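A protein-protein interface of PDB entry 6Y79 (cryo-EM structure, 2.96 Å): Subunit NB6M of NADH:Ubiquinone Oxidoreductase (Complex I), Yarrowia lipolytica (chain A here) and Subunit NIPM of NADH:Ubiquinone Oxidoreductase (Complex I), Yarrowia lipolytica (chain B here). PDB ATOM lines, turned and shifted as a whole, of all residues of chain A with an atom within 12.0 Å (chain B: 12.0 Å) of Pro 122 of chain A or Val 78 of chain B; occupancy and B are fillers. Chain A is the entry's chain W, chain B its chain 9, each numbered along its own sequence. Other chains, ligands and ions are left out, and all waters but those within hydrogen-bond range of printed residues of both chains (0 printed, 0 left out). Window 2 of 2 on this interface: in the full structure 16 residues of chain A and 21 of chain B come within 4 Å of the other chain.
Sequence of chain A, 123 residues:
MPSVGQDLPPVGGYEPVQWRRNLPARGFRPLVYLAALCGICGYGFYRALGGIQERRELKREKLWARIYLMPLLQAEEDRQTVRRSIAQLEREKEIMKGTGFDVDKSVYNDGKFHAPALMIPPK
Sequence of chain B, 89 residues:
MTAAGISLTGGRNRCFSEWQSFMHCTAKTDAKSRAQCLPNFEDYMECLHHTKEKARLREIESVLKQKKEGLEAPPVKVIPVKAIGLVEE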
ATOM      1  N   ARG A  84      -0.831 -23.282  -4.325  1.00  0.00           N
ATOM      2  CA  ARG A  84      -0.029 -23.111  -3.116  1.00  0.00           C
ATOM      3  C   ARG A  84       0.706 -24.385  -2.728  1.00  0.00           C
ATOM      4  O   ARG A  84       1.809 -24.315  -2.173  1.00  0.00           O
ATOM      5  CB  ARG A  84      -0.903 -22.648  -1.968  1.00  0.00           C
ATOM      6  CG  ARG A  84      -1.620 -21.357  -2.241  1.00  0.00           C
ATOM      7  CD  ARG A  84      -2.538 -21.050  -1.123  1.00  0.00           C
ATOM      8  NE  ARG A  84      -1.743 -20.949   0.078  1.00  0.00           N
ATOM      9  CZ  ARG A  84      -1.435 -19.801   0.651  1.00  0.00           C
ATOM     10  NH1 ARG A  84      -0.684 -19.773   1.735  1.00  0.00           N
ATOM     11  NH2 ARG A  84      -1.892 -18.680   0.131  1.00  0.00           N
ATOM     12  N   GLN A  88       4.714 -24.746  -2.421  1.00  0.00           N
ATOM     13  CA  GLN A  88       5.418 -25.271  -1.251  1.00  0.00           C
ATOM     14  C   GLN A  88       6.366 -26.403  -1.628  1.00  0.00           C
ATOM     15  O   GLN A  88       7.470 -26.513  -1.072  1.00  0.00           O
ATOM     16  CB  GLN A  88       4.406 -25.752  -0.213  1.00  0.00           C
ATOM     17  CG  GLN A  88       5.023 -26.266   1.071  1.00  0.00           C
ATOM     18  CD  GLN A  88       5.593 -25.155   1.914  1.00  0.00           C
ATOM     19  OE1 GLN A  88       4.979 -24.099   2.059  1.00  0.00           O
ATOM     20  NE2 GLN A  88       6.775 -25.376   2.469  1.00  0.00           N
ATOM     21  N   ARG A  91       9.263 -24.946  -3.178  1.00  0.00           N
ATOM     22  CA  ARG A  91       9.995 -24.202  -2.162  1.00  0.00           C
ATOM     23  C   ARG A  91      10.938 -25.112  -1.392  1.00  0.00           C
ATOM     24  O   ARG A  91      12.123 -24.801  -1.249  1.00  0.00           O
ATOM     25  CB  ARG A  91       9.027 -23.514  -1.211  1.00  0.00           C
ATOM     26  CG  ARG A  91       9.709 -22.664  -0.147  1.00  0.00           C
ATOM     27  CD  ARG A  91       8.742 -21.666   0.468  1.00  0.00           C
ATOM     28  NE  ARG A  91       7.698 -21.270  -0.474  1.00  0.00           N
ATOM     29  CZ  ARG A  91       6.404 -21.519  -0.302  1.00  0.00           C
ATOM     30  NH1 ARG A  91       5.526 -21.131  -1.215  1.00  0.00           N
ATOM     31  NH2 ARG A  91       5.999 -22.187   0.765  1.00  0.00           N
ATOM     32  N   ILE A  95      14.875 -25.483  -1.055  1.00  0.00           N
ATOM     33  CA  ILE A  95      15.557 -25.507   0.234  1.00  0.00           C
ATOM     34  C   ILE A  95      16.654 -26.565   0.235  1.00  0.00           C
ATOM     35  O   ILE A  95      17.813 -26.268   0.528  1.00  0.00           O
ATOM     36  CB  ILE A  95      14.556 -25.716   1.389  1.00  0.00           C
ATOM     37  CG1 ILE A  95      13.681 -24.475   1.597  1.00  0.00           C
ATOM     38  CG2 ILE A  95      15.290 -26.088   2.680  1.00  0.00           C
ATOM     39  CD1 ILE A  95      12.535 -24.692   2.553  1.00  0.00           C
ATOM     40  N   ALA A 117       0.228 -30.390   4.944  1.00  0.00           N
ATOM     41  CA  ALA A 117      -0.179 -29.820   6.214  1.00  0.00           C
ATOM     42  C   ALA A 117       1.056 -29.679   7.089  1.00  0.00           C
ATOM     43  O   ALA A 117       2.182 -29.942   6.655  1.00  0.00           O
ATOM     44  CB  ALA A 117      -1.258 -30.675   6.883  1.00  0.00           C
ATOM     45  N   LEU A 118       0.827 -29.198   8.312  1.00  0.00           N
ATOM     46  CA  LEU A 118       1.775 -29.279   9.424  1.00  0.00           C
ATOM     47  C   LEU A 118       3.038 -28.453   9.171  1.00  0.00           C
ATOM     48  O   LEU A 118       4.151 -28.902   9.434  1.00  0.00           O
ATOM     49  CB  LEU A 118       2.118 -30.734   9.754  1.00  0.00           C
ATOM     50  CG  LEU A 118       1.241 -31.451  10.778  1.00  0.00           C
ATOM     51  CD1 LEU A 118      -0.177 -31.653  10.311  1.00  0.00           C
ATOM     52  CD2 LEU A 118       1.861 -32.773  11.056  1.00  0.00           C
ATOM     53  N   MET A 119       2.862 -27.228   8.691  1.00  0.00           N
ATOM     54  CA  MET A 119       3.992 -26.368   8.373  1.00  0.00           C
ATOM     55  C   MET A 119       4.690 -25.867   9.633  1.00  0.00           C
ATOM     56  O   MET A 119       4.138 -25.895  10.733  1.00  0.00           O
ATOM     57  CB  MET A 119       3.515 -25.174   7.567  1.00  0.00           C
ATOM     58  CG  MET A 119       2.391 -24.450   8.247  1.00  0.00           C
ATOM     59  SD  MET A 119       2.073 -22.877   7.466  1.00  0.00           S
ATOM     60  CE  MET A 119       3.542 -21.933   7.806  1.00  0.00           C
ATOM     61  N   ILE A 120       5.912 -25.395   9.455  1.00  0.00           N
ATOM     62  CA  ILE A 120       6.682 -24.797  10.552  1.00  0.00           C
ATOM     63  C   ILE A 120       6.164 -23.389  10.809  1.00  0.00           C
ATOM     64  O   ILE A 120       5.913 -22.650   9.845  1.00  0.00           O
ATOM     65  CB  ILE A 120       8.159 -24.778  10.183  1.00  0.00           C
ATOM     66  CG1 ILE A 120       8.489 -26.077   9.456  1.00  0.00           C
ATOM     67  CG2 ILE A 120       9.041 -24.562  11.415  1.00  0.00           C
ATOM     68  CD1 ILE A 120       9.738 -26.020   8.660  1.00  0.00           C
ATOM     69  N   PRO A 121       5.989 -22.970  12.059  1.00  0.00           N
ATOM     70  CA  PRO A 121       5.514 -21.606  12.330  1.00  0.00           C
ATOM     71  C   PRO A 121       6.545 -20.560  11.939  1.00  0.00           C
ATOM     72  O   PRO A 121       7.750 -20.733  12.177  1.00  0.00           O
ATOM     73  CB  PRO A 121       5.270 -21.609  13.847  1.00  0.00           C
ATOM     74  CG  PRO A 121       6.024 -22.782  14.358  1.00  0.00           C
ATOM     75  CD  PRO A 121       5.964 -23.799  13.272  1.00  0.00           C
ATOM     76  N   PRO A 122       6.109 -19.458  11.315  1.00  0.00           N
ATOM     77  CA  PRO A 122       6.969 -18.352  10.882  1.00  0.00           C
ATOM     78  C   PRO A 122       7.259 -17.349  11.998  1.00  0.00           C
ATOM     79  O   PRO A 122       8.288 -16.673  11.958  1.00  0.00           O
ATOM     80  CB  PRO A 122       6.149 -17.703   9.780  1.00  0.00           C
ATOM     81  CG  PRO A 122       4.761 -17.960  10.210  1.00  0.00           C
ATOM     82  CD  PRO A 122       4.716 -19.264  10.880  1.00  0.00           C
ATOM     83  N   GLU B  61      13.518 -29.404   8.193  1.00  0.00           N
ATOM     84  CA  GLU B  61      13.779 -28.262   9.062  1.00  0.00           C
ATOM     85  C   GLU B  61      15.173 -28.346   9.656  1.00  0.00           C
ATOM     86  O   GLU B  61      15.808 -27.305   9.889  1.00  0.00           O
ATOM     87  CB  GLU B  61      12.706 -28.191  10.153  1.00  0.00           C
ATOM     88  CG  GLU B  61      12.552 -26.865  10.900  1.00  0.00           C
ATOM     89  CD  GLU B  61      13.369 -26.816  12.160  1.00  0.00           C
ATOM     90  OE1 GLU B  61      13.741 -27.895  12.645  1.00  0.00           O
ATOM     91  OE2 GLU B  61      13.587 -25.702  12.727  1.00  0.00           O
ATOM     92  N   LEU B  64      17.182 -26.612   6.882  1.00  0.00           N
ATOM     93  CA  LEU B  64      17.033 -25.160   6.717  1.00  0.00           C
ATOM     94  C   LEU B  64      17.525 -24.378   7.935  1.00  0.00           C
ATOM     95  O   LEU B  64      17.745 -23.163   7.840  1.00  0.00           O
ATOM     96  CB  LEU B  64      15.591 -24.777   6.388  1.00  0.00           C
ATOM     97  CG  LEU B  64      14.323 -24.881   7.208  1.00  0.00           C
ATOM     98  CD1 LEU B  64      14.064 -23.665   8.107  1.00  0.00           C
ATOM     99  CD2 LEU B  64      13.231 -25.012   6.178  1.00  0.00           C
ATOM    100  N   LEU B  71      16.440 -19.069   2.595  1.00  0.00           N
ATOM    101  CA  LEU B  71      15.339 -19.272   1.657  1.00  0.00           C
ATOM    102  C   LEU B  71      15.559 -18.395   0.434  1.00  0.00           C
ATOM    103  O   LEU B  71      15.640 -17.169   0.550  1.00  0.00           O
ATOM    104  CB  LEU B  71      13.992 -18.977   2.327  1.00  0.00           C
ATOM    105  CG  LEU B  71      12.658 -19.238   1.624  1.00  0.00           C
ATOM    106  CD1 LEU B  71      11.664 -19.793   2.631  1.00  0.00           C
ATOM    107  CD2 LEU B  71      12.093 -17.962   0.999  1.00  0.00           C
ATOM    108  N   PRO B  74      10.099 -18.219  -3.923  1.00  0.00           N
ATOM    109  CA  PRO B  74       8.900 -17.444  -3.672  1.00  0.00           C
ATOM    110  C   PRO B  74       8.463 -17.615  -2.229  1.00  0.00           C
ATOM    111  O   PRO B  74       7.996 -18.696  -1.840  1.00  0.00           O
ATOM    112  CB  PRO B  74       7.895 -18.064  -4.644  1.00  0.00           C
ATOM    113  CG  PRO B  74       8.722 -18.499  -5.778  1.00  0.00           C
ATOM    114  CD  PRO B  74       9.979 -19.022  -5.152  1.00  0.00           C
ATOM    115  N   PRO B  75       8.587 -16.579  -1.407  1.00  0.00           N
ATOM    116  CA  PRO B  75       8.374 -16.744   0.033  1.00  0.00           C
ATOM    117  C   PRO B  75       6.889 -16.741   0.375  1.00  0.00           C
ATOM    118  O   PRO B  75       6.025 -16.582  -0.486  1.00  0.00           O
ATOM    119  CB  PRO B  75       9.086 -15.526   0.625  1.00  0.00           C
ATOM    120  CG  PRO B  75       8.874 -14.462  -0.415  1.00  0.00           C
ATOM    121  CD  PRO B  75       8.810 -15.167  -1.764  1.00  0.00           C
ATOM    122  N   VAL B  76       6.595 -16.946   1.658  1.00  0.00           N
ATOM    123  CA  VAL B  76       5.231 -16.851   2.162  1.00  0.00           C
ATOM    124  C   VAL B  76       5.146 -15.701   3.159  1.00  0.00           C
ATOM    125  O   VAL B  76       6.049 -15.490   3.984  1.00  0.00           O
ATOM    126  CB  VAL B  76       4.727 -18.176   2.761  1.00  0.00           C
ATOM    127  CG1 VAL B  76       4.616 -19.224   1.671  1.00  0.00           C
ATOM    128  CG2 VAL B  76       5.600 -18.689   3.900  1.00  0.00           C
ATOM    129  N   LYS B  77       4.070 -14.929   3.032  1.00  0.00           N
ATOM    130  CA  LYS B  77       3.811 -13.733   3.825  1.00  0.00           C
ATOM    131  C   LYS B  77       2.938 -14.103   5.000  1.00  0.00           C
ATOM    132  O   LYS B  77       2.140 -15.019   4.892  1.00  0.00           O
ATOM    133  CB  LYS B  77       3.117 -12.694   2.978  1.00  0.00           C
ATOM    134  CG  LYS B  77       2.650 -11.395   3.616  1.00  0.00           C
ATOM    135  CD  LYS B  77       3.764 -10.347   3.662  1.00  0.00           C
ATOM    136  CE  LYS B  77       3.166  -9.008   3.942  1.00  0.00           C
ATOM    137  NZ  LYS B  77       2.405  -9.161   5.193  1.00  0.00           N
ATOM    138  N   VAL B  78       3.126 -13.454   6.122  1.00  0.00           N
ATOM    139  CA  VAL B  78       2.144 -13.509   7.204  1.00  0.00           C
ATOM    140  C   VAL B  78       1.466 -12.153   7.330  1.00  0.00           C
ATOM    141  O   VAL B  78       2.120 -11.110   7.224  1.00  0.00           O
ATOM    142  CB  VAL B  78       2.816 -13.952   8.515  1.00  0.00           C
ATOM    143  CG1 VAL B  78       1.941 -13.720   9.739  1.00  0.00           C
ATOM    144  CG2 VAL B  78       3.122 -15.392   8.374  1.00  0.00           C
ATOM    145  N   ILE B  79       0.146 -12.161   7.491  1.00  0.00           N
ATOM    146  CA  ILE B  79      -0.622 -10.934   7.662  1.00  0.00           C
ATOM    147  C   ILE B  79      -1.222 -10.874   9.059  1.00  0.00           C
ATOM    148  O   ILE B  79      -1.362 -11.914   9.718  1.00  0.00           O
ATOM    149  CB  ILE B  79      -1.723 -10.842   6.600  1.00  0.00           C
ATOM    150  CG1 ILE B  79      -2.452 -12.178   6.514  1.00  0.00           C
ATOM    151  CG2 ILE B  79      -1.146 -10.422   5.269  1.00  0.00           C
ATOM    152  CD1 ILE B  79      -3.618 -12.183   5.629  1.00  0.00           C
ATOM    153  N   PRO B  80      -1.564  -9.691   9.555  1.00  0.00           N
ATOM    154  CA  PRO B  80      -2.548  -9.613  10.632  1.00  0.00           C
ATOM    155  C   PRO B  80      -3.936  -9.892  10.083  1.00  0.00           C
ATOM    156  O   PRO B  80      -4.207  -9.740   8.891  1.00  0.00           O
ATOM    157  CB  PRO B  80      -2.428  -8.170  11.130  1.00  0.00           C
ATOM    158  CG  PRO B  80      -1.915  -7.418   9.950  1.00  0.00           C
ATOM    159  CD  PRO B  80      -0.998  -8.368   9.225  1.00  0.00           C
ATOM    160  N   VAL B  81      -4.833 -10.270  10.998  1.00  0.00           N
ATOM    161  CA  VAL B  81      -6.217 -10.576  10.638  1.00  0.00           C
ATOM    162  C   VAL B  81      -6.970  -9.319  10.205  1.00  0.00           C
ATOM    163  O   VAL B  81      -8.045  -9.403   9.601  1.00  0.00           O
ATOM    164  CB  VAL B  81      -6.904 -11.292  11.817  1.00  0.00           C
ATOM    165  CG1 VAL B  81      -6.027 -12.431  12.315  1.00  0.00           C
ATOM    166  CG2 VAL B  81      -7.183 -10.320  12.943  1.00  0.00           C
ATOM    167  N   LYS B  82      -6.410  -8.145  10.483  1.00  0.00           N
ATOM    168  CA  LYS B  82      -6.945  -6.859  10.078  1.00  0.00           C
ATOM    169  C   LYS B  82      -6.736  -6.576   8.590  1.00  0.00           C
ATOM    170  O   LYS B  82      -7.287  -5.601   8.078  1.00  0.00           O
ATOM    171  CB  LYS B  82      -6.287  -5.763  10.910  1.00  0.00           C
ATOM    172  CG  LYS B  82      -6.240  -6.058  12.402  1.00  0.00           C
ATOM    173  CD  LYS B  82      -4.835  -5.833  12.976  1.00  0.00           C
ATOM    174  CE  LYS B  82      -4.711  -6.538  14.327  1.00  0.00           C
ATOM    175  NZ  LYS B  82      -3.338  -6.976  14.701  1.00  0.00           N
ATOM    176  N   ALA B  83      -5.926  -7.378   7.897  1.00  0.00           N
ATOM    177  CA  ALA B  83      -5.347  -6.998   6.607  1.00  0.00           C
ATOM    178  C   ALA B  83      -5.314  -8.173   5.632  1.00  0.00           C
ATOM    179  O   ALA B  83      -4.284  -8.469   5.021  1.00  0.00           O
ATOM    180  CB  ALA B  83      -3.954  -6.437   6.822  1.00  0.00           C
ATOM    181  N   ILE B  84      -6.435  -8.885   5.480  1.00  0.00           N
ATOM    182  CA  ILE B  84      -6.461 -10.037   4.573  1.00  0.00           C
ATOM    183  C   ILE B  84      -6.531  -9.577   3.115  1.00  0.00           C
ATOM    184  O   ILE B  84      -5.838 -10.111   2.236  1.00  0.00           O
ATOM    185  CB  ILE B  84      -7.610 -10.995   4.952  1.00  0.00           C
ATOM    186  CG1 ILE B  84      -7.279 -11.641   6.298  1.00  0.00           C
ATOM    187  CG2 ILE B  84      -7.885 -12.056   3.877  1.00  0.00           C
ATOM    188  CD1 ILE B  84      -8.230 -12.712   6.750  1.00  0.00           C
ATOM    189  N   GLY B  85      -7.321  -8.544   2.845  1.00  0.00           N
ATOM    190  CA  GLY B  85      -7.402  -8.047   1.491  1.00  0.00           C
ATOM    191  C   GLY B  85      -6.985  -6.600   1.332  1.00  0.00           C
ATOM    192  O   GLY B  85      -7.641  -5.868   0.594  1.00  0.00           O
ATOM    193  N   LEU B  86      -5.897  -6.177   1.983  1.00  0.00           N
ATOM    194  CA  LEU B  86      -5.614  -4.750   2.148  1.00  0.00           C
ATOM    195  C   LEU B  86      -5.256  -4.072   0.826  1.00  0.00           C
ATOM    196  O   LEU B  86      -5.974  -3.180   0.363  1.00  0.00           O
ATOM    197  CB  LEU B  86      -4.494  -4.558   3.175  1.00  0.00           C
ATOM    198  CG  LEU B  86      -4.179  -3.117   3.575  1.00  0.00           C
ATOM    199  CD1 LEU B  86      -5.410  -2.429   4.142  1.00  0.00           C
ATOM    200  CD2 LEU B  86      -3.054  -3.102   4.594  1.00  0.00           C
ATOM    201  N   VAL B  87      -4.157  -4.484   0.199  1.00  0.00           N
ATOM    202  CA  VAL B  87      -3.752  -3.847  -1.047  1.00  0.00           C
ATOM    203  C   VAL B  87      -4.559  -4.414  -2.207  1.00  0.00           C
ATOM    204  O   VAL B  87      -5.539  -3.813  -2.643  1.00  0.00           O
ATOM    205  CB  VAL B  87      -2.249  -4.002  -1.314  1.00  0.00           C
ATOM    206  CG1 VAL B  87      -1.857  -5.473  -1.329  1.00  0.00           C
ATOM    207  CG2 VAL B  87      -1.887  -3.332  -2.624  1.00  0.00           C
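Printed residues of chain B within 4 Å of Arg 91 of chain A: Pro 74 (2.9 Å) and Val 76 (3.4 Å). Printed residues of chain A within 4 Å of Glu 61 of chain B: Ile 120 (3.7 Å). Printed residues of chain A within 4 Å of Leu 64 of chain B: Ile 95. Of the printed residues of chain A, Pro 74 of chain B touches Arg 91 (2.9 Å). Of the printed residues of chain A, Val 76 of chain B touches Arg 91. No residue of chain A comes within 4 Å of Lys 77 of chain B. Val 78 of chain B touches just one residue of chain A: Pro 122. No residue of chain A comes within 4 Å of Pro 80 of chain B.
O of Pro 74 of chain B lies within hydrogen-bond range of NE of Arg 91 of chain A (2.9 Å).
Val 76 of chain B touches Arg 91 of chain A (CG1 to NH2, 3.4 Å). Ile 95 of chain A touches Leu 64 of chain B (CD1 to CD2, 3.7 Å). Glu 61 of chain B touches Ile 120 of chain A (CG to CD1, 3.7 Å). Pro 122 of chain A touches Val 78 of chain B (CG to CG2, 3.6 Å).
The side-chain amide oxygen of Gln 88 of chain A lies within hydrogen-bond range of the guanidinium group of Arg 91 of chain A.
Printed residues of chain B that touch a printed residue of chain A: Glu 61, Leu 64, Pro 74, Val 76 and Val 78. Along chain B the printed residues that touch a printed residue of chain A span positions 61 to 78. Among the printed residues, 5 pairs touch across the chains.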
